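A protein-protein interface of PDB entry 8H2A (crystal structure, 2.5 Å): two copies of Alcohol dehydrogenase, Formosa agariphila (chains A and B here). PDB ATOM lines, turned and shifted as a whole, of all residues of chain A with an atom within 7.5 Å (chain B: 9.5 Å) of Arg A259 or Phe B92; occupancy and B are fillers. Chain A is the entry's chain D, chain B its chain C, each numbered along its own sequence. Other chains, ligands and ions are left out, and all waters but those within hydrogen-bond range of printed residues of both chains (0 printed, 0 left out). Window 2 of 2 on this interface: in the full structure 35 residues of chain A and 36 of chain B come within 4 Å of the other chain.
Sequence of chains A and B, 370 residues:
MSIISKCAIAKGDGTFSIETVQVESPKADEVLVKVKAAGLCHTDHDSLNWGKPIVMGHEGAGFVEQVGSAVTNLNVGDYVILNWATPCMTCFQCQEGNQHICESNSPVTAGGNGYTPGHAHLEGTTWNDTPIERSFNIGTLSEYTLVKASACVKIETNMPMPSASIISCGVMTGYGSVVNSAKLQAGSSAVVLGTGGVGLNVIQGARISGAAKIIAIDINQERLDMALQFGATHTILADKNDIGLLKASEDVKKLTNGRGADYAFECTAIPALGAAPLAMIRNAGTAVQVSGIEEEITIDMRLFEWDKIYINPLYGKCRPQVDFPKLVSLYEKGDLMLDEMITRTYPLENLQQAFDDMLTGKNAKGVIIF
Of the 18 printed residues of chain A, 4 touch a printed residue of chain B. Hydrophobic or aromatic side chains of chain A within 4 Å of the printed part of chain B: Ala A284. Of the 17 printed residues of chain B, 6 touch a printed residue of chain A. Among the printed residues, 9 pairs touch across the chains. Among the printed residues, Asp or Glu carboxylates within 4 Å of a Lys or Arg side-chain nitrogen of the other chain: Arg A259 with Glu B103 (3.2 Å).
The side-chain carboxylate of Glu B103 lies within salt-bridge range of the guanidinium group of Arg A259 (3.2 Å). NE2 of Gln B93 is in hydrogen-bond range of O of Asn A283 (2.7 Å).
Among the printed residues, pairs that only touch across the chains: Arg A259 with Phe B92 (3.3 Å), Arg A282 with Phe B92 (3.3 Å), Arg A282 with Gln B93 (3.7 Å), Asn A283 with Ile B101 (3.8 Å), Asn A283 with Thr B109 (3.7 Å), Ala A284 with Asn B98 (3.4 Å) and Ala A284 with Ile B101 (3.9 Å).
The guanidinium group (NH2) of Arg A282 lies within hydrogen-bond range of the backbone carbonyl oxygen (O) of Ala A284 (2.9 Å). The side-chain carboxylate (OD1) of Asp A262 is in salt-bridge range of the guanidinium group (NE) of Arg A282, 2.6 Å away. O of Cys B102 is in hydrogen-bond range of OG1 of Thr B109 (2.8 Å). The backbone NH of Glu B103 lies close to the side-chain sulfur of Cys B91 (3.5 Å). The backbone carbonyl oxygen (O) of Ala A261 lies within hydrogen-bond range of the backbone NH (N) of Arg A282, at 3.1 Å. O of Gln B93 sits at hydrogen-bond distance from N of Asn B98 (2.7 Å).
No position is printed for both chains.
Of the printed residues of chain B, Arg A259 touches Phe B92 (3.3 Å) and Glu B103 (3.2 Å). No residue of chain B comes within 4 Å of Gly A260. Printed residues of chain B within 4 Å of Asn A283: Gln B93 (2.7 Å), Ile B101 (3.8 Å) and Thr B109 (3.7 Å). Of the printed residues of chain B, Ala A284 touches Asn B98 (3.4 Å) and Ile B101 (3.9 Å). Of the printed residues of chain A, Thr B109 touches Asn A283. Of the printed residues of chain A, Glu B103 touches Arg A259 (3.2 Å). The nearest residue of chain B that does not touch Arg A259 is Gln B93 (4.7 Å). The nearest residue of chain A that does not touch Phe B92 is Asp A262 (4.2 Å). The nearest printed residue of chain A that does not touch Glu B103 is Arg A282 (5.9 Å).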
ATOM      1  N   SER A 249       5.252   9.208  18.738  1.00  0.00           N
ATOM      2  CA  SER A 249       5.670  10.499  19.265  1.00  0.00           C
ATOM      3  C   SER A 249       5.641  10.490  20.784  1.00  0.00           C
ATOM      4  O   SER A 249       6.511  11.087  21.424  1.00  0.00           O
ATOM      5  CB  SER A 249       4.807  11.641  18.739  1.00  0.00           C
ATOM      6  OG  SER A 249       3.619  11.770  19.498  1.00  0.00           O
ATOM      7  N   VAL A 252       8.580   8.871  22.001  1.00  0.00           N
ATOM      8  CA  VAL A 252       9.692   9.804  21.840  1.00  0.00           C
ATOM      9  C   VAL A 252       9.754  10.775  23.016  1.00  0.00           C
ATOM     10  O   VAL A 252      10.840  11.090  23.522  1.00  0.00           O
ATOM     11  CB  VAL A 252       9.580  10.538  20.488  1.00  0.00           C
ATOM     12  CG1 VAL A 252      10.512  11.752  20.433  1.00  0.00           C
ATOM     13  CG2 VAL A 252       9.909   9.581  19.343  1.00  0.00           C
ATOM     14  N   LYS A 253       8.593  11.234  23.496  1.00  0.00           N
ATOM     15  CA  LYS A 253       8.579  12.167  24.617  1.00  0.00           C
ATOM     16  C   LYS A 253       9.066  11.511  25.888  1.00  0.00           C
ATOM     17  O   LYS A 253       9.679  12.176  26.726  1.00  0.00           O
ATOM     18  CB  LYS A 253       7.183  12.749  24.821  1.00  0.00           C
ATOM     19  CG  LYS A 253       6.751  13.653  23.675  1.00  0.00           C
ATOM     20  CD  LYS A 253       5.378  14.256  23.877  1.00  0.00           C
ATOM     21  CE  LYS A 253       5.130  15.350  22.843  1.00  0.00           C
ATOM     22  NZ  LYS A 253       4.081  16.343  23.271  1.00  0.00           N
ATOM     23  N   LYS A 254       8.827  10.209  26.052  1.00  0.00           N
ATOM     24  CA  LYS A 254       9.345   9.526  27.233  1.00  0.00           C
ATOM     25  C   LYS A 254      10.870   9.470  27.203  1.00  0.00           C
ATOM     26  O   LYS A 254      11.522   9.670  28.235  1.00  0.00           O
ATOM     27  CB  LYS A 254       8.743   8.118  27.342  1.00  0.00           C
ATOM     28  CG  LYS A 254       7.222   8.101  27.506  1.00  0.00           C
ATOM     29  CD  LYS A 254       6.712   6.676  27.428  1.00  0.00           C
ATOM     30  CE  LYS A 254       5.185   6.574  27.536  1.00  0.00           C
ATOM     31  NZ  LYS A 254       4.585   7.113  28.803  1.00  0.00           N
ATOM     32  N   THR A 256      12.795  11.639  25.811  1.00  0.00           N
ATOM     33  CA  THR A 256      13.360  12.982  25.674  1.00  0.00           C
ATOM     34  C   THR A 256      12.835  13.950  26.745  1.00  0.00           C
ATOM     35  O   THR A 256      12.670  15.148  26.477  1.00  0.00           O
ATOM     36  CB  THR A 256      13.109  13.534  24.267  1.00  0.00           C
ATOM     37  OG1 THR A 256      11.701  13.594  24.010  1.00  0.00           O
ATOM     38  CG2 THR A 256      13.777  12.651  23.226  1.00  0.00           C
ATOM     39  N   ASN A 257      12.545  13.432  27.947  1.00  0.00           N
ATOM     40  CA  ASN A 257      12.327  14.212  29.168  1.00  0.00           C
ATOM     41  C   ASN A 257      10.966  14.907  29.215  1.00  0.00           C
ATOM     42  O   ASN A 257      10.811  15.934  29.875  1.00  0.00           O
ATOM     43  CB  ASN A 257      13.426  15.257  29.372  1.00  0.00           C
ATOM     44  CG  ASN A 257      14.813  14.664  29.315  1.00  0.00           C
ATOM     45  OD1 ASN A 257      15.597  14.986  28.419  1.00  0.00           O
ATOM     46  ND2 ASN A 257      15.140  13.820  30.287  1.00  0.00           N
ATOM     47  N   GLY A 258       9.951  14.344  28.568  1.00  0.00           N
ATOM     48  CA  GLY A 258       8.806  15.142  28.175  1.00  0.00           C
ATOM     49  C   GLY A 258       9.179  15.861  26.893  1.00  0.00           C
ATOM     50  O   GLY A 258       9.966  15.355  26.090  1.00  0.00           O
ATOM     51  N   ARG A 259       8.664  17.074  26.725  1.00  0.00           N
ATOM     52  CA  ARG A 259       9.205  17.913  25.652  1.00  0.00           C
ATOM     53  C   ARG A 259       9.131  17.179  24.317  1.00  0.00           C
ATOM     54  O   ARG A 259       8.059  16.733  23.903  1.00  0.00           O
ATOM     55  CB  ARG A 259      10.662  18.308  25.948  1.00  0.00           C
ATOM     56  CG  ARG A 259      10.822  19.537  26.826  1.00  0.00           C
ATOM     57  CD  ARG A 259      12.073  20.365  26.476  1.00  0.00           C
ATOM     58  NE  ARG A 259      13.291  19.785  27.019  1.00  0.00           N
ATOM     59  CZ  ARG A 259      13.594  19.811  28.306  1.00  0.00           C
ATOM     60  NH1 ARG A 259      14.719  19.261  28.735  1.00  0.00           N
ATOM     61  NH2 ARG A 259      12.751  20.381  29.158  1.00  0.00           N
ATOM     62  N   GLY A 260      10.277  17.012  23.678  1.00  0.00           N
ATOM     63  CA  GLY A 260      10.380  16.194  22.491  1.00  0.00           C
ATOM     64  C   GLY A 260      11.837  16.076  22.119  1.00  0.00           C
ATOM     65  O   GLY A 260      12.718  16.316  22.945  1.00  0.00           O
ATOM     66  N   ALA A 261      12.101  15.727  20.866  1.00  0.00           N
ATOM     67  CA  ALA A 261      13.480  15.761  20.392  1.00  0.00           C
ATOM     68  C   ALA A 261      13.852  17.156  19.864  1.00  0.00           C
ATOM     69  O   ALA A 261      13.010  17.902  19.341  1.00  0.00           O
ATOM     70  CB  ALA A 261      13.702  14.697  19.316  1.00  0.00           C
ATOM     71  N   ASP A 262      15.132  17.514  20.024  1.00  0.00           N
ATOM     72  CA  ASP A 262      15.610  18.799  19.504  1.00  0.00           C
ATOM     73  C   ASP A 262      15.591  18.842  17.980  1.00  0.00           C
ATOM     74  O   ASP A 262      15.524  19.928  17.397  1.00  0.00           O
ATOM     75  CB  ASP A 262      17.022  19.097  20.005  1.00  0.00           C
ATOM     76  CG  ASP A 262      17.105  19.166  21.512  1.00  0.00           C
ATOM     77  OD1 ASP A 262      16.074  19.420  22.153  1.00  0.00           O
ATOM     78  OD2 ASP A 262      18.199  18.952  22.060  1.00  0.00           O
ATOM     79  N   ALA A 279       5.550  16.388  15.407  1.00  0.00           N
ATOM     80  CA  ALA A 279       5.093  15.697  16.602  1.00  0.00           C
ATOM     81  C   ALA A 279       6.255  15.172  17.430  1.00  0.00           C
ATOM     82  O   ALA A 279       6.094  14.981  18.633  1.00  0.00           O
ATOM     83  CB  ALA A 279       4.154  14.549  16.228  1.00  0.00           C
ATOM     84  N   MET A 280       7.422  14.956  16.817  1.00  0.00           N
ATOM     85  CA  MET A 280       8.584  14.371  17.488  1.00  0.00           C
ATOM     86  C   MET A 280       9.421  15.390  18.260  1.00  0.00           C
ATOM     87  O   MET A 280      10.378  15.006  18.945  1.00  0.00           O
ATOM     88  CB  MET A 280       9.468  13.665  16.452  1.00  0.00           C
ATOM     89  CG  MET A 280       8.712  12.644  15.621  1.00  0.00           C
ATOM     90  SD  MET A 280       7.975  11.291  16.600  1.00  0.00           S
ATOM     91  CE  MET A 280       6.897  10.596  15.352  1.00  0.00           C
ATOM     92  N   ILE A 281       9.068  16.662  18.190  1.00  0.00           N
ATOM     93  CA  ILE A 281       9.992  17.746  18.494  1.00  0.00           C
ATOM     94  C   ILE A 281       9.477  18.656  19.596  1.00  0.00           C
ATOM     95  O   ILE A 281       8.277  18.940  19.683  1.00  0.00           O
ATOM     96  CB  ILE A 281      10.314  18.509  17.193  1.00  0.00           C
ATOM     97  CG1 ILE A 281      11.368  17.763  16.391  1.00  0.00           C
ATOM     98  CG2 ILE A 281      10.447  19.991  17.343  1.00  0.00           C
ATOM     99  CD1 ILE A 281      11.475  18.348  15.037  1.00  0.00           C
ATOM    100  N   ARG A 282      10.406  19.088  20.443  1.00  0.00           N
ATOM    101  CA  ARG A 282      10.120  20.103  21.438  1.00  0.00           C
ATOM    102  C   ARG A 282       9.810  21.434  20.759  1.00  0.00           C
ATOM    103  O   ARG A 282      10.171  21.665  19.609  1.00  0.00           O
ATOM    104  CB  ARG A 282      11.306  20.287  22.386  1.00  0.00           C
ATOM    105  CG  ARG A 282      12.576  20.862  21.709  1.00  0.00           C
ATOM    106  CD  ARG A 282      13.552  21.375  22.767  1.00  0.00           C
ATOM    107  NE  ARG A 282      14.867  21.736  22.240  1.00  0.00           N
ATOM    108  CZ  ARG A 282      15.195  22.899  21.674  1.00  0.00           C
ATOM    109  NH1 ARG A 282      16.434  23.075  21.250  1.00  0.00           N
ATOM    110  NH2 ARG A 282      14.320  23.883  21.526  1.00  0.00           N
ATOM    111  N   ASN A 283       9.109  22.307  21.476  1.00  0.00           N
ATOM    112  CA  ASN A 283       8.944  23.666  20.987  1.00  0.00           C
ATOM    113  C   ASN A 283      10.311  24.274  20.767  1.00  0.00           C
ATOM    114  O   ASN A 283      11.196  24.139  21.623  1.00  0.00           O
ATOM    115  CB  ASN A 283       8.141  24.516  21.970  1.00  0.00           C
ATOM    116  CG  ASN A 283       6.643  24.227  21.896  1.00  0.00           C
ATOM    117  OD1 ASN A 283       6.148  23.687  20.901  1.00  0.00           O
ATOM    118  ND2 ASN A 283       5.921  24.597  22.942  1.00  0.00           N
ATOM    119  N   ALA A 284      10.482  24.896  19.591  1.00  0.00           N
ATOM    120  CA  ALA A 284      11.730  25.505  19.127  1.00  0.00           C
ATOM    121  C   ALA A 284      12.778  24.467  18.723  1.00  0.00           C
ATOM    122  O   ALA A 284      13.978  24.740  18.808  1.00  0.00           O
ATOM    123  CB  ALA A 284      12.311  26.446  20.186  1.00  0.00           C
ATOM    124  N   LYS A 308       8.887  25.858  15.939  1.00  0.00           N
ATOM    125  CA  LYS A 308       9.422  24.685  15.269  1.00  0.00           C
ATOM    126  C   LYS A 308       9.726  25.062  13.829  1.00  0.00           C
ATOM    127  O   LYS A 308       8.858  25.564  13.108  1.00  0.00           O
ATOM    128  CB  LYS A 308       8.434  23.524  15.330  1.00  0.00           C
ATOM    129  CG  LYS A 308       7.840  23.303  16.714  1.00  0.00           C
ATOM    130  CD  LYS A 308       6.910  22.094  16.764  1.00  0.00           C
ATOM    131  CE  LYS A 308       6.658  21.655  18.202  1.00  0.00           C
ATOM    132  NZ  LYS A 308       5.428  20.794  18.335  1.00  0.00           N
ATOM    133  N   CYS B  88      10.132  32.509  33.872  1.00  0.00           N
ATOM    134  CA  CYS B  88      10.726  31.989  35.103  1.00  0.00           C
ATOM    135  C   CYS B  88      12.260  32.121  35.137  1.00  0.00           C
ATOM    136  O   CYS B  88      12.840  32.193  36.229  1.00  0.00           O
ATOM    137  CB  CYS B  88      10.314  30.522  35.322  1.00  0.00           C
ATOM    138  SG  CYS B  88      11.294  29.245  34.451  1.00  0.00           S
ATOM    139  N   MET B  89      12.928  32.153  33.981  1.00  0.00           N
ATOM    140  CA  MET B  89      14.382  32.316  33.809  1.00  0.00           C
ATOM    141  C   MET B  89      15.223  31.081  34.156  1.00  0.00           C
ATOM    142  O   MET B  89      16.482  31.168  34.054  1.00  0.00           O
ATOM    143  CB  MET B  89      14.928  33.506  34.615  1.00  0.00           C
ATOM    144  CG  MET B  89      14.070  34.767  34.515  1.00  0.00           C
ATOM    145  SD  MET B  89      14.038  35.302  32.784  1.00  0.00           S
ATOM    146  CE  MET B  89      15.137  36.734  32.871  1.00  0.00           C
ATOM    147  N   THR B  90      14.608  29.937  34.533  1.00  0.00           N
ATOM    148  CA  THR B  90      15.331  28.749  35.000  1.00  0.00           C
ATOM    149  C   THR B  90      15.008  27.458  34.237  1.00  0.00           C
ATOM    150  O   THR B  90      15.773  26.487  34.340  1.00  0.00           O
ATOM    151  CB  THR B  90      15.060  28.506  36.497  1.00  0.00           C
ATOM    152  OG1 THR B  90      13.659  28.646  36.767  1.00  0.00           O
ATOM    153  CG2 THR B  90      15.816  29.486  37.333  1.00  0.00           C
ATOM    154  N   CYS B  91      13.920  27.411  33.471  1.00  0.00           N
ATOM    155  CA  CYS B  91      13.604  26.185  32.760  1.00  0.00           C
ATOM    156  C   CYS B  91      14.452  26.027  31.497  1.00  0.00           C
ATOM    157  O   CYS B  91      15.332  26.834  31.168  1.00  0.00           O
ATOM    158  CB  CYS B  91      12.122  26.139  32.413  1.00  0.00           C
ATOM    159  SG  CYS B  91      11.590  27.405  31.219  1.00  0.00           S
ATOM    160  N   PHE B  92      14.160  24.949  30.782  1.00  0.00           N
ATOM    161  CA  PHE B  92      14.924  24.588  29.599  1.00  0.00           C
ATOM    162  C   PHE B  92      14.841  25.689  28.562  1.00  0.00           C
ATOM    163  O   PHE B  92      15.863  26.247  28.152  1.00  0.00           O
ATOM    164  CB  PHE B  92      14.405  23.266  29.042  1.00  0.00           C
ATOM    165  CG  PHE B  92      15.058  22.851  27.781  1.00  0.00           C
ATOM    166  CD1 PHE B  92      16.201  22.068  27.806  1.00  0.00           C
ATOM    167  CD2 PHE B  92      14.525  23.217  26.562  1.00  0.00           C
ATOM    168  CE1 PHE B  92      16.803  21.660  26.629  1.00  0.00           C
ATOM    169  CE2 PHE B  92      15.117  22.814  25.388  1.00  0.00           C
ATOM    170  CZ  PHE B  92      16.259  22.030  25.420  1.00  0.00           C
ATOM    171  N   GLN B  93      13.617  26.046  28.163  1.00  0.00           N
ATOM    172  CA  GLN B  93      13.430  27.077  27.148  1.00  0.00           C
ATOM    173  C   GLN B  93      14.055  28.414  27.564  1.00  0.00           C
ATOM    174  O   GLN B  93      14.648  29.109  26.728  1.00  0.00           O
ATOM    175  CB  GLN B  93      11.937  27.243  26.831  1.00  0.00           C
ATOM    176  CG  GLN B  93      11.329  26.059  26.060  1.00  0.00           C
ATOM    177  CD  GLN B  93      12.083  25.713  24.771  1.00  0.00           C
ATOM    178  OE1 GLN B  93      12.870  26.516  24.263  1.00  0.00           O
ATOM    179  NE2 GLN B  93      11.828  24.513  24.233  1.00  0.00           N
ATOM    180  N   CYS B  94      13.945  28.781  28.851  1.00  0.00           N
ATOM    181  CA  CYS B  94      14.476  30.063  29.300  1.00  0.00           C
ATOM    182  C   CYS B  94      15.996  30.088  29.220  1.00  0.00           C
ATOM    183  O   CYS B  94      16.596  31.120  28.888  1.00  0.00           O
ATOM    184  CB  CYS B  94      14.010  30.356  30.724  1.00  0.00           C
ATOM    185  SG  CYS B  94      12.326  31.033  30.900  1.00  0.00           S
ATOM    186  N   GLN B  95      16.642  28.962  29.519  1.00  0.00           N
ATOM    187  CA  GLN B  95      18.097  28.915  29.435  1.00  0.00           C
ATOM    188  C   GLN B  95      18.569  28.814  27.992  1.00  0.00           C
ATOM    189  O   GLN B  95      19.705  29.184  27.688  1.00  0.00           O
ATOM    190  CB  GLN B  95      18.631  27.753  30.276  1.00  0.00           C
ATOM    191  CG  GLN B  95      18.173  27.846  31.738  1.00  0.00           C
ATOM    192  CD  GLN B  95      19.108  27.169  32.685  1.00  0.00           C
ATOM    193  OE1 GLN B  95      20.292  27.052  32.401  1.00  0.00           O
ATOM    194  NE2 GLN B  95      18.589  26.717  33.823  1.00  0.00           N
ATOM    195  N   GLU B  96      17.719  28.320  27.100  1.00  0.00           N
ATOM    196  CA  GLU B  96      17.950  28.501  25.680  1.00  0.00           C
ATOM    197  C   GLU B  96      17.749  29.948  25.244  1.00  0.00           C
ATOM    198  O   GLU B  96      18.174  30.310  24.139  1.00  0.00           O
ATOM    199  CB  GLU B  96      17.014  27.586  24.893  1.00  0.00           C
ATOM    200  CG  GLU B  96      17.292  26.114  25.150  1.00  0.00           C
ATOM    201  CD  GLU B  96      18.670  25.683  24.654  1.00  0.00           C
ATOM    202  OE1 GLU B  96      19.315  24.904  25.382  1.00  0.00           O
ATOM    203  OE2 GLU B  96      19.087  26.099  23.543  1.00  0.00           O
ATOM    204  N   GLY B  97      17.118  30.781  26.080  1.00  0.00           N
ATOM    205  CA  GLY B  97      16.756  32.124  25.683  1.00  0.00           C
ATOM    206  C   GLY B  97      15.349  32.278  25.141  1.00  0.00           C
ATOM    207  O   GLY B  97      14.958  33.397  24.770  1.00  0.00           O
ATOM    208  N   ASN B  98      14.570  31.204  25.092  1.00  0.00           N
ATOM    209  CA  ASN B  98      13.211  31.288  24.580  1.00  0.00           C
ATOM    210  C   ASN B  98      12.230  31.596  25.713  1.00  0.00           C
ATOM    211  O   ASN B  98      11.320  30.836  26.007  1.00  0.00           O
ATOM    212  CB  ASN B  98      12.841  29.996  23.864  1.00  0.00           C
ATOM    213  CG  ASN B  98      13.751  29.690  22.678  1.00  0.00           C
ATOM    214  OD1 ASN B  98      14.267  30.597  22.008  1.00  0.00           O
ATOM    215  ND2 ASN B  98      13.918  28.400  22.389  1.00  0.00           N
ATOM    216  N   GLN B  99      12.428  32.754  26.344  1.00  0.00           N
ATOM    217  CA  GLN B  99      11.553  33.197  27.429  1.00  0.00           C
ATOM    218  C   GLN B  99      10.091  33.303  27.020  1.00  0.00           C
ATOM    219  O   GLN B  99       9.232  33.444  27.895  1.00  0.00           O
ATOM    220  CB  GLN B  99      12.002  34.559  27.952  1.00  0.00           C
ATOM    221  CG  GLN B  99      13.401  34.597  28.511  1.00  0.00           C
ATOM    222  CD  GLN B  99      13.795  35.991  28.956  1.00  0.00           C
ATOM    223  OE1 GLN B  99      12.938  36.854  29.150  1.00  0.00           O
ATOM    224  NE2 GLN B  99      15.092  36.221  29.124  1.00  0.00           N
ATOM    225  N   ILE B 101       8.343  30.951  25.261  1.00  0.00           N
ATOM    226  CA  ILE B 101       7.741  29.638  25.453  1.00  0.00           C
ATOM    227  C   ILE B 101       8.211  29.049  26.779  1.00  0.00           C
ATOM    228  O   ILE B 101       8.577  27.870  26.849  1.00  0.00           O
ATOM    229  CB  ILE B 101       8.077  28.685  24.290  1.00  0.00           C
ATOM    230  CG1 ILE B 101       9.576  28.668  24.020  1.00  0.00           C
ATOM    231  CG2 ILE B 101       7.375  29.109  23.030  1.00  0.00           C
ATOM    232  CD1 ILE B 101       9.965  27.644  22.998  1.00  0.00           C
ATOM    233  N   CYS B 102       8.203  29.863  27.834  1.00  0.00           N
ATOM    234  CA  CYS B 102       8.530  29.391  29.175  1.00  0.00           C
ATOM    235  C   CYS B 102       7.694  28.176  29.548  1.00  0.00           C
ATOM    236  O   CYS B 102       6.463  28.235  29.527  1.00  0.00           O
ATOM    237  CB  CYS B 102       8.307  30.504  30.200  1.00  0.00           C
ATOM    238  SG  CYS B 102       8.773  30.017  31.882  1.00  0.00           S
ATOM    239  N   GLU B 103       8.370  27.078  29.906  1.00  0.00           N
ATOM    240  CA  GLU B 103       7.689  25.820  30.178  1.00  0.00           C
ATOM    241  C   GLU B 103       6.950  25.821  31.510  1.00  0.00           C
ATOM    242  O   GLU B 103       6.089  24.965  31.720  1.00  0.00           O
ATOM    243  CB  GLU B 103       8.689  24.666  30.130  1.00  0.00           C
ATOM    244  CG  GLU B 103       9.519  24.660  28.865  1.00  0.00           C
ATOM    245  CD  GLU B 103      10.357  23.410  28.695  1.00  0.00           C
ATOM    246  OE1 GLU B 103      10.832  22.851  29.719  1.00  0.00           O
ATOM    247  OE2 GLU B 103      10.547  22.992  27.527  1.00  0.00           O
ATOM    248  N   SER B 104       7.229  26.772  32.401  1.00  0.00           N
ATOM    249  CA  SER B 104       6.550  26.819  33.691  1.00  0.00           C
ATOM    250  C   SER B 104       5.608  28.003  33.869  1.00  0.00           C
ATOM    251  O   SER B 104       4.579  27.859  34.541  1.00  0.00           O
ATOM    252  CB  SER B 104       7.577  26.828  34.826  1.00  0.00           C
ATOM    253  OG  SER B 104       8.470  25.736  34.676  1.00  0.00           O
ATOM    254  N   THR B 109       2.171  28.004  26.923  1.00  0.00           N
ATOM    255  CA  THR B 109       2.852  26.714  26.889  1.00  0.00           C
ATOM    256  C   THR B 109       2.847  25.968  28.220  1.00  0.00           C
ATOM    257  O   THR B 109       3.102  24.756  28.225  1.00  0.00           O
ATOM    258  CB  THR B 109       4.297  26.891  26.404  1.00  0.00           C
ATOM    259  OG1 THR B 109       4.935  27.917  27.168  1.00  0.00           O
ATOM    260  CG2 THR B 109       4.329  27.311  24.945  1.00  0.00           C
